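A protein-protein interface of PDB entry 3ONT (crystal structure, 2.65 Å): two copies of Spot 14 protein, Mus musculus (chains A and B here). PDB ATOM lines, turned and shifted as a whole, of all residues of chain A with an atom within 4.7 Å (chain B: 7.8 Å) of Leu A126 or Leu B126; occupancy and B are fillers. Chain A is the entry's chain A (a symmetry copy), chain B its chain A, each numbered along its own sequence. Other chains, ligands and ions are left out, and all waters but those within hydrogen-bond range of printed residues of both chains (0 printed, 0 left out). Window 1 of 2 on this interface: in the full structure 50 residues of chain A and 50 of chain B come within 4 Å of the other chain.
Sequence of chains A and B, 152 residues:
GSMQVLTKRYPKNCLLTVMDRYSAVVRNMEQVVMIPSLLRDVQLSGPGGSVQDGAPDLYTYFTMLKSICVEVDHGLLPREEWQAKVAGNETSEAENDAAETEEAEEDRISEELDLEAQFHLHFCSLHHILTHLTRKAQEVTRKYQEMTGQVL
O of His B127 lies within hydrogen-bond range of OG1 of Thr B131, at 3.2 Å. The side-chain hydroxyl of Ser B125 lies within hydrogen-bond range of the backbone carbonyl oxygen of Leu B121 (2.7 Å).
N of Leu A15 lies within hydrogen-bond range of O of Leu B76 (2.8 Å). NE2 of His B122 is in hydrogen-bond range of OG of Ser A125 (3.3 Å). A ring nitrogen (NE2) of His A122 is in hydrogen-bond range of the side-chain hydroxyl of Ser B125, at 3.3 Å. A ring nitrogen (ND1) of His A122 sits at hydrogen-bond distance from a ring nitrogen (ND1) of His B122, 2.9 Å away. The backbone NH (N) of Leu B15 sits at hydrogen-bond distance from the backbone carbonyl oxygen (O) of Leu A76, at 2.8 Å.
Among the printed residues, merely in contact across the chains: Leu A126 with Phe B119, Phe A119 with Leu B126, Leu A130 with Met B19, His A127 with Val B18, Leu A126 with His B122, His A122 with Leu B126, Leu A15 with His B127, His A127 with Leu B15, Leu A130 with Val B18, Leu A15 with Leu B126, Leu A126 with Leu B15, Leu A126 with Leu B126, Leu A130 with Phe B119, Phe A119 with Leu B130, Leu A126 with Phe B123, Phe A123 with Leu B126, Ile A129 with His B122 and His A122 with Ile B129.
Of chain B, only Leu B15 (3.6 Å), Phe B119 (3.4 Å), His B122 (3.5 Å), Phe B123 (3.8 Å) and Leu B126 (3.7 Å) come within 4 Å of Leu A126. Of chain A, only Leu A15, Phe A119, His A122, Phe A123 and Leu A126 come within 4 Å of Leu B126. Printed residues of chain B within 4 Å of Phe A123: Leu B126. Printed residues of chain A within 4 Å of Leu B130: Phe A119 (3.7 Å). Printed residues of chain A within 4 Å of His B127: Leu A15. Printed residues of chain A within 4 Å of Ile B129: His A122 (3.9 Å). Of the printed residues of chain A, Met B19 touches Leu A130. Leu B121 touches none of the printed residues of chain A. The nearest printed residue of chain A that does not touch Ser B125 is Leu A15 (6.4 Å).
Of the 12 printed residues of chain A, 10 touch a printed residue of chain B. Of the 23 printed residues of chain B, 12 touch a printed residue of chain A. Printed residues of chain B that touch a printed residue of chain A: Leu B15, Val B18, Met B19, Leu B76, Phe B119, His B122, Phe B123, Ser B125, Leu B126, His B127, Ile B129 and Leu B130. Among the printed residues, 23 pairs touch across the chains.
Leu A15 touches Leu B76, and with the chains exchanged Leu A76 touches Leu B15. Leu A15 touches His B127, and with the chains exchanged His A127 touches Leu B15. Phe A123 touches Leu B126, and with the chains exchanged Leu A126 touches Phe B123. Leu B126 touches its own counterpart, Leu A126.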
ATOM      1  N   LEU A  15     -18.267  19.101  18.936  1.00  0.00           N
ATOM      2  CA  LEU A  15     -18.861  20.236  19.652  1.00  0.00           C
ATOM      3  C   LEU A  15     -19.918  20.974  18.827  1.00  0.00           C
ATOM      4  O   LEU A  15     -20.996  21.316  19.342  1.00  0.00           O
ATOM      5  CB  LEU A  15     -17.786  21.227  20.126  1.00  0.00           C
ATOM      6  CG  LEU A  15     -18.330  22.518  20.765  1.00  0.00           C
ATOM      7  CD1 LEU A  15     -18.514  22.321  22.251  1.00  0.00           C
ATOM      8  CD2 LEU A  15     -17.470  23.750  20.492  1.00  0.00           C
ATOM      9  N   LEU A  76     -22.036  32.324  20.139  1.00  0.00           N
ATOM     10  CA  LEU A  76     -21.233  32.664  21.337  1.00  0.00           C
ATOM     11  C   LEU A  76     -20.452  33.994  21.202  1.00  0.00           C
ATOM     12  O   LEU A  76     -19.261  34.010  20.854  1.00  0.00           O
ATOM     13  CB  LEU A  76     -20.325  31.482  21.804  1.00  0.00           C
ATOM     14  CG  LEU A  76     -20.827  30.024  21.943  1.00  0.00           C
ATOM     15  CD1 LEU A  76     -19.748  29.080  22.386  1.00  0.00           C
ATOM     16  CD2 LEU A  76     -21.990  29.916  22.890  1.00  0.00           C
ATOM     17  N   PHE A 119     -19.973  27.552  31.730  1.00  0.00           N
ATOM     18  CA  PHE A 119     -20.126  27.560  30.287  1.00  0.00           C
ATOM     19  C   PHE A 119     -19.558  28.855  29.753  1.00  0.00           C
ATOM     20  O   PHE A 119     -18.722  28.859  28.845  1.00  0.00           O
ATOM     21  CB  PHE A 119     -21.605  27.423  29.907  1.00  0.00           C
ATOM     22  CG  PHE A 119     -21.888  27.635  28.446  1.00  0.00           C
ATOM     23  CD1 PHE A 119     -21.654  26.615  27.516  1.00  0.00           C
ATOM     24  CD2 PHE A 119     -22.428  28.837  27.994  1.00  0.00           C
ATOM     25  CE1 PHE A 119     -21.927  26.796  26.133  1.00  0.00           C
ATOM     26  CE2 PHE A 119     -22.707  29.036  26.616  1.00  0.00           C
ATOM     27  CZ  PHE A 119     -22.451  28.012  25.689  1.00  0.00           C
ATOM     28  N   HIS A 122     -15.674  29.031  29.928  1.00  0.00           N
ATOM     29  CA  HIS A 122     -15.175  28.240  28.816  1.00  0.00           C
ATOM     30  C   HIS A 122     -15.327  28.889  27.449  1.00  0.00           C
ATOM     31  O   HIS A 122     -14.314  29.104  26.772  1.00  0.00           O
ATOM     32  CB  HIS A 122     -15.802  26.870  28.852  1.00  0.00           C
ATOM     33  CG  HIS A 122     -15.427  26.105  30.077  1.00  0.00           C
ATOM     34  ND1 HIS A 122     -14.130  26.052  30.548  1.00  0.00           N
ATOM     35  CD2 HIS A 122     -16.172  25.385  30.945  1.00  0.00           C
ATOM     36  CE1 HIS A 122     -14.089  25.322  31.647  1.00  0.00           C
ATOM     37  NE2 HIS A 122     -15.317  24.909  31.911  1.00  0.00           N
ATOM     38  N   PHE A 123     -16.555  29.236  27.043  1.00  0.00           N
ATOM     39  CA  PHE A 123     -16.726  29.762  25.689  1.00  0.00           C
ATOM     40  C   PHE A 123     -15.971  31.058  25.486  1.00  0.00           C
ATOM     41  O   PHE A 123     -15.431  31.278  24.419  1.00  0.00           O
ATOM     42  CB  PHE A 123     -18.203  29.731  25.161  1.00  0.00           C
ATOM     43  CG  PHE A 123     -19.008  31.015  25.328  1.00  0.00           C
ATOM     44  CD1 PHE A 123     -18.701  32.169  24.615  1.00  0.00           C
ATOM     45  CD2 PHE A 123     -20.148  31.029  26.157  1.00  0.00           C
ATOM     46  CE1 PHE A 123     -19.485  33.357  24.763  1.00  0.00           C
ATOM     47  CE2 PHE A 123     -20.977  32.217  26.320  1.00  0.00           C
ATOM     48  CZ  PHE A 123     -20.637  33.379  25.617  1.00  0.00           C
ATOM     49  N   CYS A 124     -15.884  31.886  26.519  1.00  0.00           N
ATOM     50  CA  CYS A 124     -15.128  33.134  26.421  1.00  0.00           C
ATOM     51  C   CYS A 124     -13.628  32.890  26.276  1.00  0.00           C
ATOM     52  O   CYS A 124     -12.940  33.621  25.553  1.00  0.00           O
ATOM     53  CB  CYS A 124     -15.359  34.029  27.640  1.00  0.00           C
ATOM     54  SG  CYS A 124     -16.794  35.080  27.516  1.00  0.00           S
ATOM     55  N   SER A 125     -13.095  31.903  26.990  1.00  0.00           N
ATOM     56  CA  SER A 125     -11.659  31.714  26.884  1.00  0.00           C
ATOM     57  C   SER A 125     -11.258  31.023  25.593  1.00  0.00           C
ATOM     58  O   SER A 125     -10.197  31.316  25.064  1.00  0.00           O
ATOM     59  CB  SER A 125     -10.975  31.161  28.150  1.00  0.00           C
ATOM     60  OG  SER A 125     -11.835  30.459  29.003  1.00  0.00           O
ATOM     61  N   LEU A 126     -12.119  30.159  25.062  1.00  0.00           N
ATOM     62  CA  LEU A 126     -11.952  29.685  23.694  1.00  0.00           C
ATOM     63  C   LEU A 126     -11.855  30.858  22.735  1.00  0.00           C
ATOM     64  O   LEU A 126     -10.925  30.942  21.926  1.00  0.00           O
ATOM     65  CB  LEU A 126     -13.120  28.826  23.267  1.00  0.00           C
ATOM     66  CG  LEU A 126     -13.126  27.376  23.714  1.00  0.00           C
ATOM     67  CD1 LEU A 126     -14.111  26.632  22.846  1.00  0.00           C
ATOM     68  CD2 LEU A 126     -11.721  26.781  23.559  1.00  0.00           C
ATOM     69  N   HIS A 127     -12.807  31.771  22.835  1.00  0.00           N
ATOM     70  CA  HIS A 127     -12.858  32.935  21.963  1.00  0.00           C
ATOM     71  C   HIS A 127     -11.543  33.691  22.075  1.00  0.00           C
ATOM     72  O   HIS A 127     -10.984  34.119  21.068  1.00  0.00           O
ATOM     73  CB  HIS A 127     -14.065  33.835  22.329  1.00  0.00           C
ATOM     74  CG  HIS A 127     -14.297  34.980  21.383  1.00  0.00           C
ATOM     75  ND1 HIS A 127     -13.537  36.135  21.403  1.00  0.00           N
ATOM     76  CD2 HIS A 127     -15.209  35.154  20.397  1.00  0.00           C
ATOM     77  CE1 HIS A 127     -13.967  36.965  20.467  1.00  0.00           C
ATOM     78  NE2 HIS A 127     -14.982  36.394  19.842  1.00  0.00           N
ATOM     79  N   HIS A 128     -11.047  33.837  23.298  1.00  0.00           N
ATOM     80  CA  HIS A 128      -9.869  34.652  23.544  1.00  0.00           C
ATOM     81  C   HIS A 128      -8.606  33.933  23.051  1.00  0.00           C
ATOM     82  O   HIS A 128      -7.700  34.549  22.485  1.00  0.00           O
ATOM     83  CB  HIS A 128      -9.791  35.019  25.027  1.00  0.00           C
ATOM     84  CG  HIS A 128      -8.698  35.990  25.371  1.00  0.00           C
ATOM     85  ND1 HIS A 128      -8.379  36.312  26.676  1.00  0.00           N
ATOM     86  CD2 HIS A 128      -7.841  36.696  24.592  1.00  0.00           C
ATOM     87  CE1 HIS A 128      -7.385  37.186  26.685  1.00  0.00           C
ATOM     88  NE2 HIS A 128      -7.030  37.429  25.434  1.00  0.00           N
ATOM     89  N   ILE A 129      -8.556  32.623  23.229  1.00  0.00           N
ATOM     90  CA  ILE A 129      -7.415  31.879  22.733  1.00  0.00           C
ATOM     91  C   ILE A 129      -7.336  31.985  21.190  1.00  0.00           C
ATOM     92  O   ILE A 129      -6.315  32.432  20.653  1.00  0.00           O
ATOM     93  CB  ILE A 129      -7.401  30.429  23.243  1.00  0.00           C
ATOM     94  CG1 ILE A 129      -6.972  30.401  24.724  1.00  0.00           C
ATOM     95  CG2 ILE A 129      -6.477  29.581  22.380  1.00  0.00           C
ATOM     96  CD1 ILE A 129      -7.485  29.195  25.480  1.00  0.00           C
ATOM     97  N   LEU A 130      -8.416  31.630  20.494  1.00  0.00           N
ATOM     98  CA  LEU A 130      -8.410  31.645  19.027  1.00  0.00           C
ATOM     99  C   LEU A 130      -8.112  33.045  18.454  1.00  0.00           C
ATOM    100  O   LEU A 130      -7.445  33.172  17.430  1.00  0.00           O
ATOM    101  CB  LEU A 130      -9.723  31.101  18.464  1.00  0.00           C
ATOM    102  CG  LEU A 130     -10.085  29.653  18.804  1.00  0.00           C
ATOM    103  CD1 LEU A 130     -11.360  29.258  18.152  1.00  0.00           C
ATOM    104  CD2 LEU A 130      -8.994  28.711  18.366  1.00  0.00           C
ATOM    105  N   LEU B  15     -17.786  33.421  18.533  1.00  0.00           N
ATOM    106  CA  LEU B  15     -16.846  32.297  18.565  1.00  0.00           C
ATOM    107  C   LEU B  15     -16.783  31.532  17.241  1.00  0.00           C
ATOM    108  O   LEU B  15     -15.692  31.189  16.759  1.00  0.00           O
ATOM    109  CB  LEU B  15     -17.169  31.325  19.712  1.00  0.00           C
ATOM    110  CG  LEU B  15     -16.318  30.042  19.738  1.00  0.00           C
ATOM    111  CD1 LEU B  15     -15.068  30.269  20.552  1.00  0.00           C
ATOM    112  CD2 LEU B  15     -17.069  28.814  20.243  1.00  0.00           C
ATOM    113  N   VAL B  18     -15.043  33.520  14.627  1.00  0.00           N
ATOM    114  CA  VAL B  18     -13.676  33.459  15.102  1.00  0.00           C
ATOM    115  C   VAL B  18     -12.987  32.126  14.728  1.00  0.00           C
ATOM    116  O   VAL B  18     -11.837  32.127  14.262  1.00  0.00           O
ATOM    117  CB  VAL B  18     -13.631  33.747  16.636  1.00  0.00           C
ATOM    118  CG1 VAL B  18     -12.514  32.992  17.320  1.00  0.00           C
ATOM    119  CG2 VAL B  18     -13.491  35.237  16.889  1.00  0.00           C
ATOM    120  N   MET B  19     -13.702  31.013  14.909  1.00  0.00           N
ATOM    121  CA  MET B  19     -13.198  29.700  14.524  1.00  0.00           C
ATOM    122  C   MET B  19     -12.754  29.610  13.074  1.00  0.00           C
ATOM    123  O   MET B  19     -11.618  29.184  12.799  1.00  0.00           O
ATOM    124  CB  MET B  19     -14.181  28.589  14.839  1.00  0.00           C
ATOM    125  CG  MET B  19     -13.961  28.037  16.199  1.00  0.00           C
ATOM    126  SD  MET B  19     -15.408  26.932  16.872  1.00  0.00           S
ATOM    127  CE  MET B  19     -15.036  25.188  16.045  1.00  0.00           C
ATOM    128  N   VAL B  72     -10.095  22.574  15.503  1.00  0.00           N
ATOM    129  CA  VAL B  72     -11.076  23.534  15.070  1.00  0.00           C
ATOM    130  C   VAL B  72     -11.783  23.037  13.815  1.00  0.00           C
ATOM    131  O   VAL B  72     -12.970  23.253  13.664  1.00  0.00           O
ATOM    132  CB  VAL B  72     -10.417  24.897  14.806  1.00  0.00           C
ATOM    133  CG1 VAL B  72     -11.366  25.838  14.090  1.00  0.00           C
ATOM    134  CG2 VAL B  72      -9.904  25.514  16.109  1.00  0.00           C
ATOM    135  N   LEU B  76     -14.305  20.191  16.709  1.00  0.00           N
ATOM    136  CA  LEU B  76     -13.907  19.883  18.104  1.00  0.00           C
ATOM    137  C   LEU B  76     -14.502  18.558  18.639  1.00  0.00           C
ATOM    138  O   LEU B  76     -15.538  18.547  19.324  1.00  0.00           O
ATOM    139  CB  LEU B  76     -14.149  21.083  19.074  1.00  0.00           C
ATOM    140  CG  LEU B  76     -13.733  22.539  18.750  1.00  0.00           C
ATOM    141  CD1 LEU B  76     -14.101  23.502  19.840  1.00  0.00           C
ATOM    142  CD2 LEU B  76     -12.260  22.656  18.472  1.00  0.00           C
ATOM    143  N   PRO B  78     -13.819  15.422  21.175  1.00  0.00           N
ATOM    144  CA  PRO B  78     -13.041  14.930  22.326  1.00  0.00           C
ATOM    145  C   PRO B  78     -12.294  13.611  22.068  1.00  0.00           C
ATOM    146  O   PRO B  78     -12.862  12.672  21.503  1.00  0.00           O
ATOM    147  CB  PRO B  78     -14.107  14.747  23.413  1.00  0.00           C
ATOM    148  CG  PRO B  78     -15.142  15.754  23.076  1.00  0.00           C
ATOM    149  CD  PRO B  78     -15.188  15.811  21.570  1.00  0.00           C
ATOM    150  N   LEU B 115      -1.211  26.863  25.855  1.00  0.00           N
ATOM    151  CA  LEU B 115      -2.443  27.241  25.173  1.00  0.00           C
ATOM    152  C   LEU B 115      -3.179  26.080  24.525  1.00  0.00           C
ATOM    153  O   LEU B 115      -4.405  26.048  24.558  1.00  0.00           O
ATOM    154  CB  LEU B 115      -2.216  28.381  24.178  1.00  0.00           C
ATOM    155  CG  LEU B 115      -2.107  29.796  24.773  1.00  0.00           C
ATOM    156  CD1 LEU B 115      -2.330  30.843  23.707  1.00  0.00           C
ATOM    157  CD2 LEU B 115      -3.102  30.029  25.884  1.00  0.00           C
ATOM    158  N   GLN B 118      -4.878  24.217  27.461  1.00  0.00           N
ATOM    159  CA  GLN B 118      -5.959  25.064  27.937  1.00  0.00           C
ATOM    160  C   GLN B 118      -7.136  25.034  26.959  1.00  0.00           C
ATOM    161  O   GLN B 118      -8.275  24.791  27.364  1.00  0.00           O
ATOM    162  CB  GLN B 118      -5.454  26.492  28.184  1.00  0.00           C
ATOM    163  CG  GLN B 118      -4.492  26.563  29.377  1.00  0.00           C
ATOM    164  CD  GLN B 118      -3.831  27.943  29.572  1.00  0.00           C
ATOM    165  OE1 GLN B 118      -4.349  28.985  29.131  1.00  0.00           O
ATOM    166  NE2 GLN B 118      -2.680  27.949  30.255  1.00  0.00           N
ATOM    167  N   PHE B 119      -6.841  25.222  25.674  1.00  0.00           N
ATOM    168  CA  PHE B 119      -7.845  25.183  24.624  1.00  0.00           C
ATOM    169  C   PHE B 119      -8.606  23.884  24.740  1.00  0.00           C
ATOM    170  O   PHE B 119      -9.838  23.869  24.791  1.00  0.00           O
ATOM    171  CB  PHE B 119      -7.179  25.298  23.249  1.00  0.00           C
ATOM    172  CG  PHE B 119      -8.109  25.052  22.093  1.00  0.00           C
ATOM    173  CD1 PHE B 119      -8.980  26.055  21.649  1.00  0.00           C
ATOM    174  CD2 PHE B 119      -8.093  23.836  21.415  1.00  0.00           C
ATOM    175  CE1 PHE B 119      -9.855  25.843  20.552  1.00  0.00           C
ATOM    176  CE2 PHE B 119      -8.962  23.605  20.314  1.00  0.00           C
ATOM    177  CZ  PHE B 119      -9.844  24.613  19.890  1.00  0.00           C
ATOM    178  N   HIS B 120      -7.862  22.786  24.802  1.00  0.00           N
ATOM    179  CA  HIS B 120      -8.460  21.471  24.889  1.00  0.00           C
ATOM    180  C   HIS B 120      -9.342  21.355  26.133  1.00  0.00           C
ATOM    181  O   HIS B 120     -10.460  20.851  26.053  1.00  0.00           O
ATOM    182  CB  HIS B 120      -7.384  20.394  24.868  1.00  0.00           C
ATOM    183  CG  HIS B 120      -7.930  19.016  24.673  1.00  0.00           C
ATOM    184  ND1 HIS B 120      -7.970  18.080  25.686  1.00  0.00           N
ATOM    185  CD2 HIS B 120      -8.491  18.422  23.588  1.00  0.00           C
ATOM    186  CE1 HIS B 120      -8.521  16.966  25.228  1.00  0.00           C
ATOM    187  NE2 HIS B 120      -8.849  17.146  23.959  1.00  0.00           N
ATOM    188  N   LEU B 121      -8.862  21.840  27.271  1.00  0.00           N
ATOM    189  CA  LEU B 121      -9.670  21.790  28.474  1.00  0.00           C
ATOM    190  C   LEU B 121     -11.030  22.494  28.261  1.00  0.00           C
ATOM    191  O   LEU B 121     -12.079  21.898  28.482  1.00  0.00           O
ATOM    192  CB  LEU B 121      -8.940  22.405  29.661  1.00  0.00           C
ATOM    193  CG  LEU B 121      -9.845  22.709  30.873  1.00  0.00           C
ATOM    194  CD1 LEU B 121     -10.522  21.454  31.459  1.00  0.00           C
ATOM    195  CD2 LEU B 121      -9.038  23.412  31.931  1.00  0.00           C
ATOM    196  N   HIS B 122     -10.981  23.747  27.821  1.00  0.00           N
ATOM    197  CA  HIS B 122     -12.161  24.519  27.466  1.00  0.00           C
ATOM    198  C   HIS B 122     -13.099  23.841  26.480  1.00  0.00           C
ATOM    199  O   HIS B 122     -14.268  23.621  26.820  1.00  0.00           O
ATOM    200  CB  HIS B 122     -11.740  25.884  26.981  1.00  0.00           C
ATOM    201  CG  HIS B 122     -11.055  26.678  28.044  1.00  0.00           C
ATOM    202  ND1 HIS B 122     -11.536  26.753  29.337  1.00  0.00           N
ATOM    203  CD2 HIS B 122      -9.919  27.409  28.022  1.00  0.00           C
ATOM    204  CE1 HIS B 122     -10.731  27.507  30.062  1.00  0.00           C
ATOM    205  NE2 HIS B 122      -9.739  27.914  29.288  1.00  0.00           N
ATOM    206  N   PHE B 123     -12.611  23.475  25.289  1.00  0.00           N
ATOM    207  CA  PHE B 123     -13.528  22.919  24.294  1.00  0.00           C
ATOM    208  C   PHE B 123     -14.159  21.626  24.766  1.00  0.00           C
ATOM    209  O   PHE B 123     -15.321  21.389  24.492  1.00  0.00           O
ATOM    210  CB  PHE B 123     -12.977  22.924  22.825  1.00  0.00           C
ATOM    211  CG  PHE B 123     -12.317  21.636  22.346  1.00  0.00           C
ATOM    212  CD1 PHE B 123     -13.048  20.470  22.143  1.00  0.00           C
ATOM    213  CD2 PHE B 123     -10.946  21.628  22.012  1.00  0.00           C
ATOM    214  CE1 PHE B 123     -12.417  19.278  21.665  1.00  0.00           C
ATOM    215  CE2 PHE B 123     -10.275  20.436  21.509  1.00  0.00           C
ATOM    216  CZ  PHE B 123     -11.020  19.262  21.339  1.00  0.00           C
ATOM    217  N   CYS B 124     -13.419  20.821  25.516  1.00  0.00           N
ATOM    218  CA  CYS B 124     -13.971  19.579  26.055  1.00  0.00           C
ATOM    219  C   CYS B 124     -15.054  19.833  27.102  1.00  0.00           C
ATOM    220  O   CYS B 124     -16.042  19.094  27.174  1.00  0.00           O
ATOM    221  CB  CYS B 124     -12.883  18.706  26.686  1.00  0.00           C
ATOM    222  SG  CYS B 124     -12.040  17.639  25.533  1.00  0.00           S
ATOM    223  N   SER B 125     -14.863  20.840  27.950  1.00  0.00           N
ATOM    224  CA  SER B 125     -15.874  21.040  28.972  1.00  0.00           C
ATOM    225  C   SER B 125     -17.124  21.708  28.429  1.00  0.00           C
ATOM    226  O   SER B 125     -18.210  21.415  28.903  1.00  0.00           O
ATOM    227  CB  SER B 125     -15.354  21.627  30.301  1.00  0.00           C
ATOM    228  OG  SER B 125     -14.155  22.338  30.180  1.00  0.00           O
ATOM    229  N   LEU B 126     -16.981  22.553  27.412  1.00  0.00           N
ATOM    230  CA  LEU B 126     -18.136  23.000  26.645  1.00  0.00           C
ATOM    231  C   LEU B 126     -18.921  21.808  26.124  1.00  0.00           C
ATOM    232  O   LEU B 126     -20.138  21.716  26.312  1.00  0.00           O
ATOM    233  CB  LEU B 126     -17.717  23.839  25.460  1.00  0.00           C
ATOM    234  CG  LEU B 126     -17.386  25.297  25.714  1.00  0.00           C
ATOM    235  CD1 LEU B 126     -17.418  26.014  24.386  1.00  0.00           C
ATOM    236  CD2 LEU B 126     -18.418  25.903  26.673  1.00  0.00           C
ATOM    237  N   HIS B 127     -18.219  20.887  25.481  1.00  0.00           N
ATOM    238  CA  HIS B 127     -18.842  19.706  24.902  1.00  0.00           C
ATOM    239  C   HIS B 127     -19.598  18.965  25.993  1.00  0.00           C
ATOM    240  O   HIS B 127     -20.724  18.522  25.778  1.00  0.00           O
ATOM    241  CB  HIS B 127     -17.773  18.802  24.236  1.00  0.00           C
ATOM    242  CG  HIS B 127     -18.334  17.635  23.473  1.00  0.00           C
ATOM    243  ND1 HIS B 127     -18.798  16.489  24.089  1.00  0.00           N
ATOM    244  CD2 HIS B 127     -18.495  17.433  22.142  1.00  0.00           C
ATOM    245  CE1 HIS B 127     -19.226  15.635  23.174  1.00  0.00           C
ATOM    246  NE2 HIS B 127     -19.053  16.183  21.984  1.00  0.00           N
ATOM    247  N   HIS B 128     -18.985  18.850  27.166  1.00  0.00           N
ATOM    248  CA  HIS B 128     -19.550  18.050  28.240  1.00  0.00           C
ATOM    249  C   HIS B 128     -20.750  18.772  28.869  1.00  0.00           C
ATOM    250  O   HIS B 128     -21.761  18.153  29.208  1.00  0.00           O
ATOM    251  CB  HIS B 128     -18.466  17.717  29.266  1.00  0.00           C
ATOM    252  CG  HIS B 128     -18.901  16.763  30.342  1.00  0.00           C
ATOM    253  ND1 HIS B 128     -18.109  16.471  31.435  1.00  0.00           N
ATOM    254  CD2 HIS B 128     -20.043  16.048  30.507  1.00  0.00           C
ATOM    255  CE1 HIS B 128     -18.736  15.606  32.218  1.00  0.00           C
ATOM    256  NE2 HIS B 128     -19.917  15.342  31.684  1.00  0.00           N
ATOM    257  N   ILE B 129     -20.659  20.087  28.996  1.00  0.00           N
ATOM    258  CA  ILE B 129     -21.783  20.830  29.530  1.00  0.00           C
ATOM    259  C   ILE B 129     -23.009  20.693  28.596  1.00  0.00           C
ATOM    260  O   ILE B 129     -24.074  20.244  29.037  1.00  0.00           O
ATOM    261  CB  ILE B 129     -21.416  22.290  29.841  1.00  0.00           C
ATOM    262  CG1 ILE B 129     -20.564  22.354  31.124  1.00  0.00           C
ATOM    263  CG2 ILE B 129     -22.681  23.129  29.971  1.00  0.00           C
ATOM    264  CD1 ILE B 129     -19.668  23.570  31.196  1.00  0.00           C
ATOM    265  N   LEU B 130     -22.846  21.024  27.314  1.00  0.00           N
ATOM    266  CA  LEU B 130     -23.969  20.978  26.372  1.00  0.00           C
ATOM    267  C   LEU B 130     -24.585  19.569  26.257  1.00  0.00           C
ATOM    268  O   LEU B 130     -25.797  19.427  26.108  1.00  0.00           O
ATOM    269  CB  LEU B 130     -23.555  21.496  24.995  1.00  0.00           C
ATOM    270  CG  LEU B 130     -23.075  22.948  24.909  1.00  0.00           C
ATOM    271  CD1 LEU B 130     -22.752  23.318  23.505  1.00  0.00           C
ATOM    272  CD2 LEU B 130     -24.124  23.891  25.438  1.00  0.00           C
ATOM    273  N   THR B 131     -23.748  18.535  26.331  1.00  0.00           N
ATOM    274  CA  THR B 131     -24.223  17.152  26.253  1.00  0.00           C
ATOM    275  C   THR B 131     -25.082  16.823  27.468  1.00  0.00           C
ATOM    276  O   THR B 131     -26.163  16.239  27.349  1.00  0.00           O
ATOM    277  CB  THR B 131     -23.036  16.174  26.155  1.00  0.00           C
ATOM    278  OG1 THR B 131     -22.618  16.102  24.791  1.00  0.00           O
ATOM    279  CG2 THR B 131     -23.418  14.770  26.638  1.00  0.00           C
ATOM    280  N   HIS B 132     -24.581  17.195  28.641  1.00  0.00           N
ATOM    281  CA  HIS B 132     -25.313  17.025  29.881  1.00  0.00           C
ATOM    282  C   HIS B 132     -26.657  17.788  29.798  1.00  0.00           C
ATOM    283  O   HIS B 132     -27.717  17.191  29.988  1.00  0.00           O
ATOM    284  CB  HIS B 132     -24.448  17.518  31.045  1.00  0.00           C
ATOM    285  CG  HIS B 132     -25.125  17.455  32.372  1.00  0.00           C
ATOM    286  ND1 HIS B 132     -25.471  16.264  32.975  1.00  0.00           N
ATOM    287  CD2 HIS B 132     -25.517  18.435  33.217  1.00  0.00           C
ATOM    288  CE1 HIS B 132     -26.055  16.512  34.135  1.00  0.00           C
ATOM    289  NE2 HIS B 132     -26.095  17.823  34.306  1.00  0.00           N
ATOM    290  N   LEU B 133     -26.597  19.079  29.459  1.00  0.00           N
ATOM    291  CA  LEU B 133     -27.771  19.925  29.435  1.00  0.00           C
ATOM    292  C   LEU B 133     -28.808  19.532  28.366  1.00  0.00           C
ATOM    293  O   LEU B 133     -30.021  19.701  28.581  1.00  0.00           O
ATOM    294  CB  LEU B 133     -27.372  21.386  29.287  1.00  0.00           C
ATOM    295  CG  LEU B 133     -26.623  22.003  30.473  1.00  0.00           C
ATOM    296  CD1 LEU B 133     -26.364  23.470  30.199  1.00  0.00           C
ATOM    297  CD2 LEU B 133     -27.348  21.825  31.804  1.00  0.00           C
